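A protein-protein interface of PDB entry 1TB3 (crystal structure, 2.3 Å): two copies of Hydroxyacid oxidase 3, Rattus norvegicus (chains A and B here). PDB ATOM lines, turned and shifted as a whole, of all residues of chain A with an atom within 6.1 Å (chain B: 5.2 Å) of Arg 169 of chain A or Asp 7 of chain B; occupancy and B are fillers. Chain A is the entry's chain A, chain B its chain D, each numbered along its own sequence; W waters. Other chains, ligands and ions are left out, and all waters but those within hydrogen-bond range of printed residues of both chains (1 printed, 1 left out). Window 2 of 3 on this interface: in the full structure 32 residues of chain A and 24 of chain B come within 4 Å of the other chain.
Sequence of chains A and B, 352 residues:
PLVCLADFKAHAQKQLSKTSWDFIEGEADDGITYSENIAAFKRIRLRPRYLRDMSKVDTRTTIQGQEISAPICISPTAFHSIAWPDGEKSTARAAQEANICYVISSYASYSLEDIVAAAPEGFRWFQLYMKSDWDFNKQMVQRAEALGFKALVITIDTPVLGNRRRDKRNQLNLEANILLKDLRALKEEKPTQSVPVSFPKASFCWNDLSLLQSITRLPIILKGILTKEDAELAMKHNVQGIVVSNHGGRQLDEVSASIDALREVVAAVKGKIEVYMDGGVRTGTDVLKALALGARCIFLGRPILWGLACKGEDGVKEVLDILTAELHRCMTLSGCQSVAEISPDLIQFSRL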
ATOM      1  N   ARG A 164       1.220  25.934  22.944  1.00  0.00           N
ATOM      2  CA  ARG A 164       1.606  26.848  24.006  1.00  0.00           C
ATOM      3  C   ARG A 164       3.000  26.487  24.517  1.00  0.00           C
ATOM      4  O   ARG A 164       3.169  25.602  25.358  1.00  0.00           O
ATOM      5  CB  ARG A 164       0.562  26.763  25.108  1.00  0.00           C
ATOM      6  CG  ARG A 164      -0.809  27.048  24.547  1.00  0.00           C
ATOM      7  CD  ARG A 164      -1.907  26.507  25.407  1.00  0.00           C
ATOM      8  NE  ARG A 164      -3.162  26.576  24.675  1.00  0.00           N
ATOM      9  CZ  ARG A 164      -4.325  26.155  25.145  1.00  0.00           C
ATOM     10  NH1 ARG A 164      -4.395  25.632  26.364  1.00  0.00           N
ATOM     11  NH2 ARG A 164      -5.413  26.256  24.390  1.00  0.00           N
ATOM     12  N   ARG A 165       4.002  27.180  23.988  1.00  0.00           N
ATOM     13  CA  ARG A 165       5.388  26.924  24.351  1.00  0.00           C
ATOM     14  C   ARG A 165       5.646  26.846  25.849  1.00  0.00           C
ATOM     15  O   ARG A 165       6.321  25.924  26.308  1.00  0.00           O
ATOM     16  CB  ARG A 165       6.291  27.989  23.735  1.00  0.00           C
ATOM     17  CG  ARG A 165       6.198  28.048  22.231  1.00  0.00           C
ATOM     18  CD  ARG A 165       7.034  29.171  21.667  1.00  0.00           C
ATOM     19  NE  ARG A 165       6.898  29.249  20.219  1.00  0.00           N
ATOM     20  CZ  ARG A 165       7.376  30.243  19.481  1.00  0.00           C
ATOM     21  NH1 ARG A 165       8.027  31.252  20.058  1.00  0.00           N
ATOM     22  NH2 ARG A 165       7.194  30.233  18.166  1.00  0.00           N
ATOM     23  N   ARG A 166       5.117  27.804  26.607  1.00  0.00           N
ATOM     24  CA  ARG A 166       5.326  27.826  28.051  1.00  0.00           C
ATOM     25  C   ARG A 166       4.896  26.530  28.718  1.00  0.00           C
ATOM     26  O   ARG A 166       5.667  25.940  29.471  1.00  0.00           O
ATOM     27  CB  ARG A 166       4.589  29.002  28.685  1.00  0.00           C
ATOM     28  CG  ARG A 166       5.170  30.350  28.338  1.00  0.00           C
ATOM     29  CD  ARG A 166       4.374  31.465  28.987  1.00  0.00           C
ATOM     30  NE  ARG A 166       4.875  32.771  28.580  1.00  0.00           N
ATOM     31  CZ  ARG A 166       6.112  33.199  28.810  1.00  0.00           C
ATOM     32  NH1 ARG A 166       6.978  32.419  29.450  1.00  0.00           N
ATOM     33  NH2 ARG A 166       6.482  34.401  28.391  1.00  0.00           N
ATOM     34  N   ASP A 167       3.670  26.083  28.449  1.00  0.00           N
ATOM     35  CA  ASP A 167       3.204  24.838  29.044  1.00  0.00           C
ATOM     36  C   ASP A 167       4.184  23.717  28.713  1.00  0.00           C
ATOM     37  O   ASP A 167       4.558  22.947  29.601  1.00  0.00           O
ATOM     38  CB  ASP A 167       1.810  24.459  28.538  1.00  0.00           C
ATOM     39  CG  ASP A 167       0.724  25.417  29.019  1.00  0.00           C
ATOM     40  OD1 ASP A 167       1.007  26.263  29.900  1.00  0.00           O
ATOM     41  OD2 ASP A 167      -0.416  25.316  28.512  1.00  0.00           O
ATOM     42  N   LYS A 168       4.600  23.625  27.448  1.00  0.00           N
ATOM     43  CA  LYS A 168       5.549  22.581  27.036  1.00  0.00           C
ATOM     44  C   LYS A 168       6.876  22.690  27.793  1.00  0.00           C
ATOM     45  O   LYS A 168       7.388  21.691  28.293  1.00  0.00           O
ATOM     46  CB  LYS A 168       5.823  22.639  25.528  1.00  0.00           C
ATOM     47  CG  LYS A 168       4.708  22.094  24.649  1.00  0.00           C
ATOM     48  CD  LYS A 168       5.207  21.946  23.212  1.00  0.00           C
ATOM     49  CE  LYS A 168       4.215  21.229  22.310  1.00  0.00           C
ATOM     50  NZ  LYS A 168       4.773  21.045  20.937  1.00  0.00           N
ATOM     51  N   ARG A 169       7.437  23.894  27.867  1.00  0.00           N
ATOM     52  CA  ARG A 169       8.689  24.091  28.592  1.00  0.00           C
ATOM     53  C   ARG A 169       8.526  23.739  30.075  1.00  0.00           C
ATOM     54  O   ARG A 169       9.486  23.322  30.710  1.00  0.00           O
ATOM     55  CB  ARG A 169       9.193  25.539  28.441  1.00  0.00           C
ATOM     56  CG  ARG A 169      10.055  25.758  27.202  1.00  0.00           C
ATOM     57  CD  ARG A 169      10.716  27.139  27.169  1.00  0.00           C
ATOM     58  NE  ARG A 169       9.743  28.202  26.914  1.00  0.00           N
ATOM     59  CZ  ARG A 169       9.592  28.844  25.758  1.00  0.00           C
ATOM     60  NH1 ARG A 169      10.353  28.550  24.714  1.00  0.00           N
ATOM     61  NH2 ARG A 169       8.662  29.787  25.638  1.00  0.00           N
ATOM     62  N   ASN A 170       7.316  23.910  30.619  1.00  0.00           N
ATOM     63  CA  ASN A 170       7.029  23.575  32.021  1.00  0.00           C
ATOM     64  C   ASN A 170       6.523  22.121  32.067  1.00  0.00           C
ATOM     65  O   ASN A 170       6.069  21.623  33.097  1.00  0.00           O
ATOM     66  CB  ASN A 170       5.956  24.512  32.618  1.00  0.00           C
ATOM     67  CG  ASN A 170       6.314  25.997  32.497  1.00  0.00           C
ATOM     68  OD1 ASN A 170       7.482  26.383  32.550  1.00  0.00           O
ATOM     69  ND2 ASN A 170       5.293  26.838  32.355  1.00  0.00           N
ATOM     70  N   GLN A 171       6.590  21.455  30.924  1.00  0.00           N
ATOM     71  CA  GLN A 171       6.170  20.063  30.797  1.00  0.00           C
ATOM     72  C   GLN A 171       4.795  19.743  31.387  1.00  0.00           C
ATOM     73  O   GLN A 171       4.538  18.607  31.787  1.00  0.00           O
ATOM     74  CB  GLN A 171       7.230  19.162  31.432  1.00  0.00           C
ATOM     75  CG  GLN A 171       8.637  19.720  31.288  1.00  0.00           C
ATOM     76  CD  GLN A 171       9.714  18.697  31.567  1.00  0.00           C
ATOM     77  OE1 GLN A 171      10.872  19.051  31.777  1.00  0.00           O
ATOM     78  NE2 GLN A 171       9.343  17.420  31.555  1.00  0.00           N
ATOM     79  N   LEU A 172       3.915  20.743  31.422  1.00  0.00           N
ATOM     80  CA  LEU A 172       2.562  20.575  31.956  1.00  0.00           C
ATOM     81  C   LEU A 172       2.644  20.103  33.403  1.00  0.00           C
ATOM     82  O   LEU A 172       3.607  20.415  34.101  1.00  0.00           O
ATOM     83  CB  LEU A 172       1.786  19.534  31.136  1.00  0.00           C
ATOM     84  CG  LEU A 172       1.663  19.654  29.615  1.00  0.00           C
ATOM     85  CD1 LEU A 172       0.892  18.447  29.088  1.00  0.00           C
ATOM     86  CD2 LEU A 172       0.954  20.943  29.242  1.00  0.00           C
ATOM     87  N   PRO B   1      13.233  22.150  28.572  1.00  0.00           N
ATOM     88  CA  PRO B   1      13.575  21.532  27.270  1.00  0.00           C
ATOM     89  C   PRO B   1      13.434  22.534  26.113  1.00  0.00           C
ATOM     90  O   PRO B   1      12.892  23.626  26.288  1.00  0.00           O
ATOM     91  CB  PRO B   1      12.629  20.353  27.092  1.00  0.00           C
ATOM     92  CG  PRO B   1      11.420  20.817  27.909  1.00  0.00           C
ATOM     93  CD  PRO B   1      12.023  21.514  29.128  1.00  0.00           C
ATOM     94  N   LEU B   2      13.931  22.159  24.937  1.00  0.00           N
ATOM     95  CA  LEU B   2      13.854  23.019  23.756  1.00  0.00           C
ATOM     96  C   LEU B   2      12.585  22.630  23.008  1.00  0.00           C
ATOM     97  O   LEU B   2      12.527  21.562  22.396  1.00  0.00           O
ATOM     98  CB  LEU B   2      15.088  22.806  22.872  1.00  0.00           C
ATOM     99  CG  LEU B   2      16.451  22.885  23.576  1.00  0.00           C
ATOM    100  CD1 LEU B   2      17.558  22.683  22.560  1.00  0.00           C
ATOM    101  CD2 LEU B   2      16.625  24.226  24.262  1.00  0.00           C
ATOM    102  N   VAL B   3      11.575  23.497  23.045  1.00  0.00           N
ATOM    103  CA  VAL B   3      10.297  23.179  22.415  1.00  0.00           C
ATOM    104  C   VAL B   3       9.954  23.902  21.113  1.00  0.00           C
ATOM    105  O   VAL B   3       8.908  23.645  20.527  1.00  0.00           O
ATOM    106  CB  VAL B   3       9.136  23.405  23.419  1.00  0.00           C
ATOM    107  CG1 VAL B   3       9.421  22.656  24.722  1.00  0.00           C
ATOM    108  CG2 VAL B   3       8.967  24.880  23.696  1.00  0.00           C
ATOM    109  N   CYS B   4      10.817  24.804  20.658  1.00  0.00           N
ATOM    110  CA  CYS B   4      10.556  25.537  19.420  1.00  0.00           C
ATOM    111  C   CYS B   4      11.886  25.985  18.853  1.00  0.00           C
ATOM    112  O   CYS B   4      12.917  25.821  19.508  1.00  0.00           O
ATOM    113  CB  CYS B   4       9.656  26.753  19.680  1.00  0.00           C
ATOM    114  SG  CYS B   4      10.355  27.996  20.824  1.00  0.00           S
ATOM    115  N   LEU B   5      11.880  26.544  17.645  1.00  0.00           N
ATOM    116  CA  LEU B   5      13.138  26.979  17.040  1.00  0.00           C
ATOM    117  C   LEU B   5      13.806  28.120  17.818  1.00  0.00           C
ATOM    118  O   LEU B   5      15.038  28.182  17.909  1.00  0.00           O
ATOM    119  CB  LEU B   5      12.926  27.357  15.572  1.00  0.00           C
ATOM    120  CG  LEU B   5      13.114  26.207  14.558  1.00  0.00           C
ATOM    121  CD1 LEU B   5      12.109  25.092  14.796  1.00  0.00           C
ATOM    122  CD2 LEU B   5      12.967  26.750  13.135  1.00  0.00           C
ATOM    123  N   ALA B   6      13.002  29.011  18.394  1.00  0.00           N
ATOM    124  CA  ALA B   6      13.559  30.111  19.188  1.00  0.00           C
ATOM    125  C   ALA B   6      14.400  29.560  20.348  1.00  0.00           C
ATOM    126  O   ALA B   6      15.454  30.113  20.663  1.00  0.00           O
ATOM    127  CB  ALA B   6      12.442  31.000  19.726  1.00  0.00           C
ATOM    128  N   ASP B   7      13.950  28.473  20.978  1.00  0.00           N
ATOM    129  CA  ASP B   7      14.714  27.883  22.091  1.00  0.00           C
ATOM    130  C   ASP B   7      16.069  27.386  21.599  1.00  0.00           C
ATOM    131  O   ASP B   7      17.065  27.518  22.298  1.00  0.00           O
ATOM    132  CB  ASP B   7      13.976  26.704  22.734  1.00  0.00           C
ATOM    133  CG  ASP B   7      12.731  27.123  23.499  1.00  0.00           C
ATOM    134  OD1 ASP B   7      12.429  28.337  23.563  1.00  0.00           O
ATOM    135  OD2 ASP B   7      12.056  26.219  24.041  1.00  0.00           O
ATOM    136  N   PHE B   8      16.099  26.790  20.407  1.00  0.00           N
ATOM    137  CA  PHE B   8      17.358  26.308  19.843  1.00  0.00           C
ATOM    138  C   PHE B   8      18.300  27.484  19.585  1.00  0.00           C
ATOM    139  O   PHE B   8      19.520  27.363  19.748  1.00  0.00           O
ATOM    140  CB  PHE B   8      17.127  25.531  18.541  1.00  0.00           C
ATOM    141  CG  PHE B   8      16.749  24.098  18.759  1.00  0.00           C
ATOM    142  CD1 PHE B   8      15.428  23.741  19.001  1.00  0.00           C
ATOM    143  CD2 PHE B   8      17.730  23.109  18.798  1.00  0.00           C
ATOM    144  CE1 PHE B   8      15.092  22.415  19.285  1.00  0.00           C
ATOM    145  CE2 PHE B   8      17.406  21.785  19.080  1.00  0.00           C
ATOM    146  CZ  PHE B   8      16.085  21.434  19.327  1.00  0.00           C
ATOM    147  N   LYS B   9      17.737  28.622  19.191  1.00  0.00           N
ATOM    148  CA  LYS B   9      18.550  29.803  18.953  1.00  0.00           C
ATOM    149  C   LYS B   9      19.192  30.243  20.268  1.00  0.00           C
ATOM    150  O   LYS B   9      20.409  30.386  20.361  1.00  0.00           O
ATOM    151  CB  LYS B   9      17.698  30.941  18.396  1.00  0.00           C
ATOM    152  CG  LYS B   9      18.486  32.213  18.137  1.00  0.00           C
ATOM    153  CD  LYS B   9      17.580  33.349  17.705  1.00  0.00           C
ATOM    154  CE  LYS B   9      18.394  34.591  17.319  1.00  0.00           C
ATOM    155  NZ  LYS B   9      17.523  35.724  16.852  1.00  0.00           N
ATOM    156  N   ALA B  10      18.364  30.441  21.290  1.00  0.00           N
ATOM    157  CA  ALA B  10      18.844  30.872  22.605  1.00  0.00           C
ATOM    158  C   ALA B  10      19.889  29.935  23.175  1.00  0.00           C
ATOM    159  O   ALA B  10      20.886  30.374  23.740  1.00  0.00           O
ATOM    160  CB  ALA B  10      17.681  30.985  23.573  1.00  0.00           C
ATOM    161  N   HIS B  11      19.671  28.638  23.017  1.00  0.00           N
ATOM    162  CA  HIS B  11      20.603  27.661  23.543  1.00  0.00           C
ATOM    163  C   HIS B  11      21.864  27.536  22.697  1.00  0.00           C
ATOM    164  O   HIS B  11      22.962  27.378  23.230  1.00  0.00           O
ATOM    165  CB  HIS B  11      19.905  26.307  23.676  1.00  0.00           C
ATOM    166  CG  HIS B  11      20.661  25.310  24.498  1.00  0.00           C
ATOM    167  ND1 HIS B  11      21.596  24.452  23.957  1.00  0.00           N
ATOM    168  CD2 HIS B  11      20.630  25.044  25.825  1.00  0.00           C
ATOM    169  CE1 HIS B  11      22.106  23.699  24.915  1.00  0.00           C
ATOM    170  NE2 HIS B  11      21.538  24.039  26.059  1.00  0.00           N
ATOM    171  N   ALA B  12      21.711  27.625  21.380  1.00  0.00           N
ATOM    172  CA  ALA B  12      22.850  27.507  20.470  1.00  0.00           C
ATOM    173  C   ALA B  12      23.940  28.531  20.790  1.00  0.00           C
ATOM    174  O   ALA B  12      25.137  28.228  20.756  1.00  0.00           O
ATOM    175  CB  ALA B  12      22.387  27.673  19.029  1.00  0.00           C
HETATM  176  O   HOH W   1       7.874  20.963  20.610  1.00  0.00           O
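NE of Arg 165 of chain A lies close to SG of Cys 4 of chain B (3.7 Å).
The guanidinium group (NH1) of Arg 169 of chain A is in salt-bridge range of the side-chain carboxylate (OD2) of Asp 7 of chain B, 3.0 Å away.
N of Val 3 of chain B lies within hydrogen-bond range of OD2 of Asp 7 of chain B, 2.9 Å away.
The backbone NH of Ala 6 of chain B sits close to the side-chain sulfur of Cys 4 of chain B (3.7 Å).
SG of Cys 4 of chain B is in hydrogen-bond range of OD1 of Asp 7 of chain B, at 3.5 Å.
Val 3 of chain B touches Arg 165 of chain A.
Lys 168 of chain A touches Val 3 of chain B (CB to CG1, 3.7 Å).
CD of Pro 1 of chain B touches O of Arg 169 of chain A, 3.5 Å away.
Arg 169 of chain A touches Val 3 of chain B (CG to CG2, 3.8 Å).
Arg 169 of chain A touches Cys 4 of chain B.
CD of Pro 1 of chain B touches OE1 of Gln 171 of chain A (3.8 Å).
Of chain A, only Arg 169 (2.4 Å) comes within 4 Å of Asp 7 of chain B.
Of the printed residues of chain B, Arg 165 of chain A touches Val 3 and Cys 4.
Of the printed residues of chain A, Pro 1 of chain B touches Arg 169 and Gln 171.
Asp 167 of chain A touches none of the printed residues of chain B.
The nearest printed residue of chain B that does not touch Arg 169 of chain A is Leu 2 of chain B (5.8 Å).
Of the 9 printed residues of chain A, 4 touch a printed residue of chain B.
Hydrophobic or aromatic side chains of chain B that line the printed part of chain A: Pro 1 and Val 3.
No position is printed for both chains.
Of the 8 pairs that touch across the chains among the printed residues, none has its exchanged pair printed and touching as well.
Water W1 bridges O of Val 3 of chain B (2.9 Å) and NZ of Lys 168 of chain A (3.1 Å).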
